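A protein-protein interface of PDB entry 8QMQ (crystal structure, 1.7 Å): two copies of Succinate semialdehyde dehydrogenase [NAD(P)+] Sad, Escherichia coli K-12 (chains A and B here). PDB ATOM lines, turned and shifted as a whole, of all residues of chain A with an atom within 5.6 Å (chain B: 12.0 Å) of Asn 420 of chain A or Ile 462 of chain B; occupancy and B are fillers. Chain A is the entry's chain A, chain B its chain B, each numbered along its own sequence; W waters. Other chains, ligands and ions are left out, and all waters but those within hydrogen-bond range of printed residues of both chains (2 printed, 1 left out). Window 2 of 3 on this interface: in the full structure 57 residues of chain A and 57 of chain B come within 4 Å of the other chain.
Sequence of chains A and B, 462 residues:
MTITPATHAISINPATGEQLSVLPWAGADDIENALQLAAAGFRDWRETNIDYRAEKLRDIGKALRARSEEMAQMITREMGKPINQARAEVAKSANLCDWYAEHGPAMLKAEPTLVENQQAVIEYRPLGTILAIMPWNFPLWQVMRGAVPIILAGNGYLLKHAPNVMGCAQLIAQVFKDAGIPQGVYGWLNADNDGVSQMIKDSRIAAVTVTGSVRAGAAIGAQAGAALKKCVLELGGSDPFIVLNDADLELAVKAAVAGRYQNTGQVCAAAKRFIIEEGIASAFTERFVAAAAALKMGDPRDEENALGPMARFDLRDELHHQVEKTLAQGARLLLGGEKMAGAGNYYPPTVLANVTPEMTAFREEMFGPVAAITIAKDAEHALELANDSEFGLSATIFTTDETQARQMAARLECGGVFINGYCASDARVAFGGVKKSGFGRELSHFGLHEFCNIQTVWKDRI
Phe 418 of chain A touches Trp 458 of chain B (CA to O, 3.3 Å). Arg 461 of chain B touches Phe 418 of chain A (CD to CE2, 3.9 Å). Lys 459 of chain B touches Ile 419 of chain A (CA to O, 3.4 Å). Asn 420 of chain A touches Asp 460 of chain B. Ile 462 of chain B touches Asn 420 of chain A (CG2 to O, 3.7 Å). CA of Gly 421 of chain A touches O of Arg 461 of chain B, at 3.5 Å.
O of Tyr 422 of chain A lies within hydrogen-bond range of NH1 of Arg 461 of chain B, at 2.9 Å. The backbone NH (N) of Ile 419 of chain A sits at hydrogen-bond distance from the backbone carbonyl oxygen (O) of Trp 458 of chain B (2.9 Å). The backbone NH of Asp 460 of chain B sits at hydrogen-bond distance from the backbone carbonyl oxygen of Ile 419 of chain A (2.9 Å).
No residue of chain B comes within 4 Å of Thr 396 of chain A. Ile 397 of chain A touches none of the printed residues of chain B. No residue of chain B comes within 4 Å of Phe 398 of chain A. Printed residues of chain B within 4 Å of Ile 419 of chain A: Trp 458, Lys 459 and Asp 460. Asn 420 of chain A touches just these residues of chain B: Asp 460 (3.7 Å) and Ile 462 (3.7 Å). Of chain B, only Arg 461 (3.5 Å) comes within 4 Å of Gly 421 of chain A. Val 115 of chain B touches none of the printed residues of chain A. Val 457 of chain B touches none of the printed residues of chain A. Of the printed residues of chain A, Trp 458 of chain B touches Phe 418 (3.3 Å) and Ile 419 (2.9 Å). Of the printed residues of chain A, Lys 459 of chain B touches Ile 419. Of the printed residues of chain A, Asp 460 of chain B touches Ile 419 (2.9 Å) and Asn 420 (3.7 Å). Of the printed residues of chain A, Arg 461 of chain B touches Phe 418 (3.9 Å), Gly 421 (3.5 Å) and Tyr 422 (2.9 Å). Ile 462 of chain B touches one residue of chain A.
N of Ile 397 of chain A sits at hydrogen-bond distance from O of Phe 418 of chain A (2.9 Å). N of Lys 459 of chain B lies within hydrogen-bond range of O of Gln 119 of chain B (2.8 Å). NE1 of Trp 458 of chain B lies within hydrogen-bond range of OE1 of Gln 119 of chain B, 2.9 Å away. O of Thr 399 of chain A sits at hydrogen-bond distance from ND2 of Asn 420 of chain A (2.9 Å). The side-chain carboxylate (OD2) of Asp 460 of chain B is in salt-bridge range of the side-chain amino group (NZ) of Lys 459 of chain B (3.996 Å). N of Asn 420 of chain A lies within hydrogen-bond range of O of Ile 397 of chain A, 2.9 Å away.
Of the 11 printed residues of chain A, 5 touch a printed residue of chain B. Printed residues of chain A that touch a printed residue of chain B: Phe 418, Ile 419, Asn 420, Gly 421 and Tyr 422. Among the printed residues, no Asp or Glu carboxylate lies within 4 Å of a Lys or Arg side-chain nitrogen of the other chain.
No position is printed for both chains.
Water W1 bridges the side-chain carboxylate of Asp 460 of chain B (2.6 Å) and the backbone carbonyl oxygen of Asn 420 of chain A (2.8 Å). Water W2 bridges OD1 of Asp 460 of chain B and ND2 of Asn 420 of chain A.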
ATOM      1  N   LEU A 251      -2.074  -6.798  16.183  1.00  0.00           N
ATOM      2  CA  LEU A 251      -1.381  -7.735  15.305  1.00  0.00           C
ATOM      3  C   LEU A 251      -0.891  -8.949  16.083  1.00  0.00           C
ATOM      4  O   LEU A 251      -0.940 -10.079  15.576  1.00  0.00           O
ATOM      5  CB  LEU A 251      -0.213  -7.040  14.595  1.00  0.00           C
ATOM      6  CG  LEU A 251       0.579  -7.909  13.605  1.00  0.00           C
ATOM      7  CD1 LEU A 251      -0.315  -8.363  12.473  1.00  0.00           C
ATOM      8  CD2 LEU A 251       1.784  -7.157  13.053  1.00  0.00           C
ATOM      9  N   THR A 396       8.454 -16.768  18.429  1.00  0.00           N
ATOM     10  CA  THR A 396       7.946 -15.479  17.975  1.00  0.00           C
ATOM     11  C   THR A 396       8.167 -14.442  19.064  1.00  0.00           C
ATOM     12  O   THR A 396       7.997 -14.743  20.252  1.00  0.00           O
ATOM     13  CB  THR A 396       6.429 -15.542  17.626  1.00  0.00           C
ATOM     14  OG1 THR A 396       6.188 -16.563  16.652  1.00  0.00           O
ATOM     15  CG2 THR A 396       5.938 -14.203  17.061  1.00  0.00           C
ATOM     16  N   ILE A 397       8.558 -13.226  18.665  1.00  0.00           N
ATOM     17  CA  ILE A 397       8.655 -12.088  19.580  1.00  0.00           C
ATOM     18  C   ILE A 397       7.866 -10.925  19.003  1.00  0.00           C
ATOM     19  O   ILE A 397       8.087 -10.531  17.850  1.00  0.00           O
ATOM     20  CB  ILE A 397      10.110 -11.641  19.825  1.00  0.00           C
ATOM     21  CG1 ILE A 397      10.995 -12.812  20.230  1.00  0.00           C
ATOM     22  CG2 ILE A 397      10.128 -10.530  20.887  1.00  0.00           C
ATOM     23  CD1 ILE A 397      12.487 -12.468  20.153  1.00  0.00           C
ATOM     24  N   PHE A 398       6.965 -10.357  19.811  1.00  0.00           N
ATOM     25  CA  PHE A 398       6.223  -9.157  19.448  1.00  0.00           C
ATOM     26  C   PHE A 398       6.658  -8.008  20.352  1.00  0.00           C
ATOM     27  O   PHE A 398       6.448  -8.047  21.572  1.00  0.00           O
ATOM     28  CB  PHE A 398       4.710  -9.390  19.519  1.00  0.00           C
ATOM     29  CG  PHE A 398       4.098  -9.713  18.183  1.00  0.00           C
ATOM     30  CD1 PHE A 398       4.088 -11.015  17.698  1.00  0.00           C
ATOM     31  CD2 PHE A 398       3.564  -8.708  17.386  1.00  0.00           C
ATOM     32  CE1 PHE A 398       3.554 -11.308  16.454  1.00  0.00           C
ATOM     33  CE2 PHE A 398       3.028  -8.998  16.141  1.00  0.00           C
ATOM     34  CZ  PHE A 398       3.016 -10.297  15.679  1.00  0.00           C
ATOM     35  N   THR A 399       7.271  -6.996  19.747  1.00  0.00           N
ATOM     36  CA  THR A 399       7.708  -5.794  20.444  1.00  0.00           C
ATOM     37  C   THR A 399       8.052  -4.745  19.394  1.00  0.00           C
ATOM     38  O   THR A 399       8.549  -5.084  18.319  1.00  0.00           O
ATOM     39  CB  THR A 399       8.924  -6.076  21.348  1.00  0.00           C
ATOM     40  OG1 THR A 399       9.378  -4.860  21.952  1.00  0.00           O
ATOM     41  CG2 THR A 399      10.076  -6.688  20.560  1.00  0.00           C
ATOM     42  N   THR A 400       7.771  -3.480  19.699  1.00  0.00           N
ATOM     43  CA  THR A 400       8.169  -2.418  18.784  1.00  0.00           C
ATOM     44  C   THR A 400       9.637  -2.032  18.936  1.00  0.00           C
ATOM     45  O   THR A 400      10.150  -1.273  18.105  1.00  0.00           O
ATOM     46  CB  THR A 400       7.276  -1.186  18.979  1.00  0.00           C
ATOM     47  OG1 THR A 400       7.151  -0.905  20.377  1.00  0.00           O
ATOM     48  CG2 THR A 400       5.903  -1.435  18.408  1.00  0.00           C
ATOM     49  N   PHE A 418      10.668 -15.412  14.615  1.00  0.00           N
ATOM     50  CA  PHE A 418       9.822 -14.492  13.870  1.00  0.00           C
ATOM     51  C   PHE A 418       9.561 -13.265  14.727  1.00  0.00           C
ATOM     52  O   PHE A 418       9.052 -13.384  15.843  1.00  0.00           O
ATOM     53  CB  PHE A 418       8.508 -15.165  13.474  1.00  0.00           C
ATOM     54  CG  PHE A 418       8.687 -16.190  12.419  1.00  0.00           C
ATOM     55  CD1 PHE A 418       9.179 -17.449  12.740  1.00  0.00           C
ATOM     56  CD2 PHE A 418       8.426 -15.886  11.096  1.00  0.00           C
ATOM     57  CE1 PHE A 418       9.383 -18.393  11.748  1.00  0.00           C
ATOM     58  CE2 PHE A 418       8.637 -16.828  10.101  1.00  0.00           C
ATOM     59  CZ  PHE A 418       9.103 -18.079  10.431  1.00  0.00           C
ATOM     60  N   ILE A 419       9.926 -12.096  14.214  1.00  0.00           N
ATOM     61  CA  ILE A 419       9.740 -10.834  14.916  1.00  0.00           C
ATOM     62  C   ILE A 419       8.538 -10.138  14.296  1.00  0.00           C
ATOM     63  O   ILE A 419       8.514  -9.894  13.083  1.00  0.00           O
ATOM     64  CB  ILE A 419      11.003  -9.963  14.840  1.00  0.00           C
ATOM     65  CG1 ILE A 419      12.171 -10.694  15.505  1.00  0.00           C
ATOM     66  CG2 ILE A 419      10.764  -8.618  15.500  1.00  0.00           C
ATOM     67  CD1 ILE A 419      13.551 -10.036  15.276  1.00  0.00           C
ATOM     68  N   ASN A 420       7.527  -9.871  15.124  1.00  0.00           N
ATOM     69  CA  ASN A 420       6.318  -9.140  14.721  1.00  0.00           C
ATOM     70  C   ASN A 420       5.695  -9.714  13.446  1.00  0.00           C
ATOM     71  O   ASN A 420       5.334  -8.984  12.521  1.00  0.00           O
ATOM     72  CB  ASN A 420       6.609  -7.646  14.549  1.00  0.00           C
ATOM     73  CG  ASN A 420       7.121  -7.005  15.817  1.00  0.00           C
ATOM     74  OD1 ASN A 420       6.694  -7.356  16.911  1.00  0.00           O
ATOM     75  ND2 ASN A 420       8.038  -6.054  15.676  1.00  0.00           N
ATOM     76  N   GLY A 421       5.554 -11.034  13.392  1.00  0.00           N
ATOM     77  CA  GLY A 421       4.851 -11.626  12.275  1.00  0.00           C
ATOM     78  C   GLY A 421       4.414 -13.053  12.531  1.00  0.00           C
ATOM     79  O   GLY A 421       4.429 -13.525  13.669  1.00  0.00           O
ATOM     80  N   TYR A 422       4.039 -13.736  11.439  1.00  0.00           N
ATOM     81  CA  TYR A 422       3.443 -15.070  11.473  1.00  0.00           C
ATOM     82  C   TYR A 422       4.475 -16.147  11.138  1.00  0.00           C
ATOM     83  O   TYR A 422       5.001 -16.176  10.021  1.00  0.00           O
ATOM     84  CB  TYR A 422       2.289 -15.165  10.473  1.00  0.00           C
ATOM     85  CG  TYR A 422       1.099 -14.246  10.700  1.00  0.00           C
ATOM     86  CD1 TYR A 422       1.169 -12.883  10.426  1.00  0.00           C
ATOM     87  CD2 TYR A 422      -0.123 -14.767  11.119  1.00  0.00           C
ATOM     88  CE1 TYR A 422       0.052 -12.051  10.610  1.00  0.00           C
ATOM     89  CE2 TYR A 422      -1.237 -13.949  11.303  1.00  0.00           C
ATOM     90  CZ  TYR A 422      -1.143 -12.595  11.043  1.00  0.00           C
ATOM     91  OH  TYR A 422      -2.252 -11.783  11.222  1.00  0.00           O
ATOM     92  N   VAL B 115      13.784 -13.793   0.408  1.00  0.00           N
ATOM     93  CA  VAL B 115      12.553 -13.174   0.891  1.00  0.00           C
ATOM     94  C   VAL B 115      12.597 -11.675   0.626  1.00  0.00           C
ATOM     95  O   VAL B 115      13.634 -11.021   0.791  1.00  0.00           O
ATOM     96  CB  VAL B 115      12.340 -13.475   2.384  1.00  0.00           C
ATOM     97  CG1 VAL B 115      11.076 -12.756   2.914  1.00  0.00           C
ATOM     98  CG2 VAL B 115      12.231 -14.990   2.605  1.00  0.00           C
ATOM     99  N   GLU B 116      11.455 -11.126   0.210  1.00  0.00           N
ATOM    100  CA  GLU B 116      11.361  -9.723  -0.173  1.00  0.00           C
ATOM    101  C   GLU B 116      11.668  -8.782   0.996  1.00  0.00           C
ATOM    102  O   GLU B 116      11.521  -9.126   2.173  1.00  0.00           O
ATOM    103  CB  GLU B 116       9.960  -9.425  -0.714  1.00  0.00           C
ATOM    104  CG  GLU B 116       8.817  -9.734   0.276  1.00  0.00           C
ATOM    105  CD  GLU B 116       8.328 -11.188   0.230  1.00  0.00           C
ATOM    106  OE1 GLU B 116       8.969 -12.022  -0.443  1.00  0.00           O
ATOM    107  OE2 GLU B 116       7.292 -11.498   0.870  1.00  0.00           O
ATOM    108  N   ASN B 117      12.096  -7.565   0.640  1.00  0.00           N
ATOM    109  CA  ASN B 117      12.247  -6.447   1.575  1.00  0.00           C
ATOM    110  C   ASN B 117      13.267  -6.741   2.676  1.00  0.00           C
ATOM    111  O   ASN B 117      13.196  -6.155   3.762  1.00  0.00           O
ATOM    112  CB  ASN B 117      10.900  -6.053   2.188  1.00  0.00           C
ATOM    113  CG  ASN B 117       9.850  -5.732   1.139  1.00  0.00           C
ATOM    114  OD1 ASN B 117      10.173  -5.330   0.023  1.00  0.00           O
ATOM    115  ND2 ASN B 117       8.587  -5.904   1.497  1.00  0.00           N
ATOM    116  N   GLN B 118      14.213  -7.640   2.399  1.00  0.00           N
ATOM    117  CA  GLN B 118      15.249  -8.034   3.360  1.00  0.00           C
ATOM    118  C   GLN B 118      14.642  -8.376   4.721  1.00  0.00           C
ATOM    119  O   GLN B 118      15.150  -7.983   5.775  1.00  0.00           O
ATOM    120  CB  GLN B 118      16.322  -6.951   3.490  1.00  0.00           C
ATOM    121  CG  GLN B 118      17.240  -6.824   2.271  1.00  0.00           C
ATOM    122  CD  GLN B 118      18.270  -7.945   2.176  1.00  0.00           C
ATOM    123  OE1 GLN B 118      18.472  -8.704   3.126  1.00  0.00           O
ATOM    124  NE2 GLN B 118      18.931  -8.047   1.024  1.00  0.00           N
ATOM    125  N   GLN B 119      13.534  -9.116   4.692  1.00  0.00           N
ATOM    126  CA  GLN B 119      12.854  -9.501   5.921  1.00  0.00           C
ATOM    127  C   GLN B 119      13.577 -10.607   6.673  1.00  0.00           C
ATOM    128  O   GLN B 119      13.463 -10.679   7.899  1.00  0.00           O
ATOM    129  CB  GLN B 119      11.437  -9.984   5.616  1.00  0.00           C
ATOM    130  CG  GLN B 119      10.446  -8.899   5.237  1.00  0.00           C
ATOM    131  CD  GLN B 119       9.089  -9.489   4.902  1.00  0.00           C
ATOM    132  OE1 GLN B 119       8.907 -10.710   4.922  1.00  0.00           O
ATOM    133  NE2 GLN B 119       8.133  -8.629   4.585  1.00  0.00           N
ATOM    134  N   ALA B 120      14.287 -11.487   5.972  1.00  0.00           N
ATOM    135  CA  ALA B 120      14.778 -12.725   6.567  1.00  0.00           C
ATOM    136  C   ALA B 120      16.267 -12.894   6.310  1.00  0.00           C
ATOM    137  O   ALA B 120      16.734 -12.701   5.185  1.00  0.00           O
ATOM    138  CB  ALA B 120      14.013 -13.940   6.018  1.00  0.00           C
ATOM    139  N   THR B 456      17.042 -19.116  11.262  1.00  0.00           N
ATOM    140  CA  THR B 456      16.316 -18.132  10.469  1.00  0.00           C
ATOM    141  C   THR B 456      15.776 -17.046  11.391  1.00  0.00           C
ATOM    142  O   THR B 456      15.163 -17.353  12.416  1.00  0.00           O
ATOM    143  CB  THR B 456      15.165 -18.805   9.715  1.00  0.00           C
ATOM    144  OG1 THR B 456      15.691 -19.711   8.747  1.00  0.00           O
ATOM    145  CG2 THR B 456      14.278 -17.764   9.011  1.00  0.00           C
ATOM    146  N   VAL B 457      16.018 -15.780  11.047  1.00  0.00           N
ATOM    147  CA  VAL B 457      15.435 -14.648  11.757  1.00  0.00           C
ATOM    148  C   VAL B 457      14.650 -13.832  10.740  1.00  0.00           C
ATOM    149  O   VAL B 457      15.230 -13.283   9.796  1.00  0.00           O
ATOM    150  CB  VAL B 457      16.495 -13.787  12.459  1.00  0.00           C
ATOM    151  CG1 VAL B 457      15.826 -12.634  13.203  1.00  0.00           C
ATOM    152  CG2 VAL B 457      17.322 -14.639  13.430  1.00  0.00           C
ATOM    153  N   TRP B 458      13.333 -13.760  10.927  1.00  0.00           N
ATOM    154  CA  TRP B 458      12.426 -13.260   9.902  1.00  0.00           C
ATOM    155  C   TRP B 458      11.535 -12.202  10.538  1.00  0.00           C
ATOM    156  O   TRP B 458      10.755 -12.512  11.446  1.00  0.00           O
ATOM    157  CB  TRP B 458      11.598 -14.412   9.318  1.00  0.00           C
ATOM    158  CG  TRP B 458      10.810 -14.106   8.056  1.00  0.00           C
ATOM    159  CD1 TRP B 458      10.405 -12.882   7.594  1.00  0.00           C
ATOM    160  CD2 TRP B 458      10.347 -15.067   7.101  1.00  0.00           C
ATOM    161  NE1 TRP B 458       9.712 -13.030   6.402  1.00  0.00           N
ATOM    162  CE2 TRP B 458       9.664 -14.363   6.085  1.00  0.00           C
ATOM    163  CE3 TRP B 458      10.448 -16.464   7.006  1.00  0.00           C
ATOM    164  CZ2 TRP B 458       9.090 -15.006   4.991  1.00  0.00           C
ATOM    165  CZ3 TRP B 458       9.871 -17.099   5.918  1.00  0.00           C
ATOM    166  CH2 TRP B 458       9.200 -16.368   4.929  1.00  0.00           C
ATOM    167  N   LYS B 459      11.668 -10.960  10.077  1.00  0.00           N
ATOM    168  CA  LYS B 459      10.901  -9.835  10.606  1.00  0.00           C
ATOM    169  C   LYS B 459       9.732  -9.492   9.690  1.00  0.00           C
ATOM    170  O   LYS B 459       9.842  -9.571   8.464  1.00  0.00           O
ATOM    171  CB  LYS B 459      11.793  -8.600  10.782  1.00  0.00           C
ATOM    172  CG  LYS B 459      11.151  -7.472  11.594  1.00  0.00           C
ATOM    173  CD  LYS B 459      12.028  -6.207  11.622  1.00  0.00           C
ATOM    174  CE  LYS B 459      11.975  -5.460  10.287  1.00  0.00           C
ATOM    175  NZ  LYS B 459      12.694  -4.155  10.319  1.00  0.00           N
ATOM    176  N   ASP B 460       8.606  -9.108  10.300  1.00  0.00           N
ATOM    177  CA  ASP B 460       7.458  -8.542   9.575  1.00  0.00           C
ATOM    178  C   ASP B 460       6.899  -9.491   8.510  1.00  0.00           C
ATOM    179  O   ASP B 460       6.486  -9.060   7.429  1.00  0.00           O
ATOM    180  CB  ASP B 460       7.819  -7.201   8.935  1.00  0.00           C
ATOM    181  CG  ASP B 460       8.148  -6.129   9.958  1.00  0.00           C
ATOM    182  OD1 ASP B 460       7.661  -6.211  11.104  1.00  0.00           O
ATOM    183  OD2 ASP B 460       8.903  -5.199   9.610  1.00  0.00           O
ATOM    184  N   ARG B 461       6.863 -10.790   8.798  1.00  0.00           N
ATOM    185  CA  ARG B 461       6.202 -11.707   7.865  1.00  0.00           C
ATOM    186  C   ARG B 461       4.699 -11.586   8.069  1.00  0.00           C
ATOM    187  O   ARG B 461       4.106 -12.289   8.885  1.00  0.00           O
ATOM    188  CB  ARG B 461       6.663 -13.147   8.054  1.00  0.00           C
ATOM    189  CG  ARG B 461       6.016 -14.088   7.037  1.00  0.00           C
ATOM    190  CD  ARG B 461       6.438 -15.554   7.189  1.00  0.00           C
ATOM    191  NE  ARG B 461       5.742 -16.379   6.200  1.00  0.00           N
ATOM    192  CZ  ARG B 461       4.486 -16.791   6.330  1.00  0.00           C
ATOM    193  NH1 ARG B 461       3.794 -16.561   7.437  1.00  0.00           N
ATOM    194  NH2 ARG B 461       3.911 -17.451   5.329  1.00  0.00           N
ATOM    195  N   ILE B 462       4.081 -10.668   7.325  1.00  0.00           N
ATOM    196  CA  ILE B 462       2.643 -10.398   7.463  1.00  0.00           C
ATOM    197  C   ILE B 462       1.982 -10.325   6.093  1.00  0.00           C
ATOM    198  O   ILE B 462       2.645 -10.392   5.055  1.00  0.00           O
ATOM    199  CB  ILE B 462       2.375  -9.095   8.248  1.00  0.00           C
ATOM    200  CG1 ILE B 462       2.932  -7.888   7.495  1.00  0.00           C
ATOM    201  CG2 ILE B 462       2.943  -9.160   9.672  1.00  0.00           C
ATOM    202  CD1 ILE B 462       2.635  -6.567   8.187  1.00  0.00           C
ATOM    203  OXT ILE B 462       0.758 -10.191   5.994  1.00  0.00           O
HETATM  204  O   HOH W   1       5.077  -6.349  11.492  1.00  0.00           O
HETATM  205  O   HOH W   2       8.909  -5.003  13.162  1.00  0.00           O
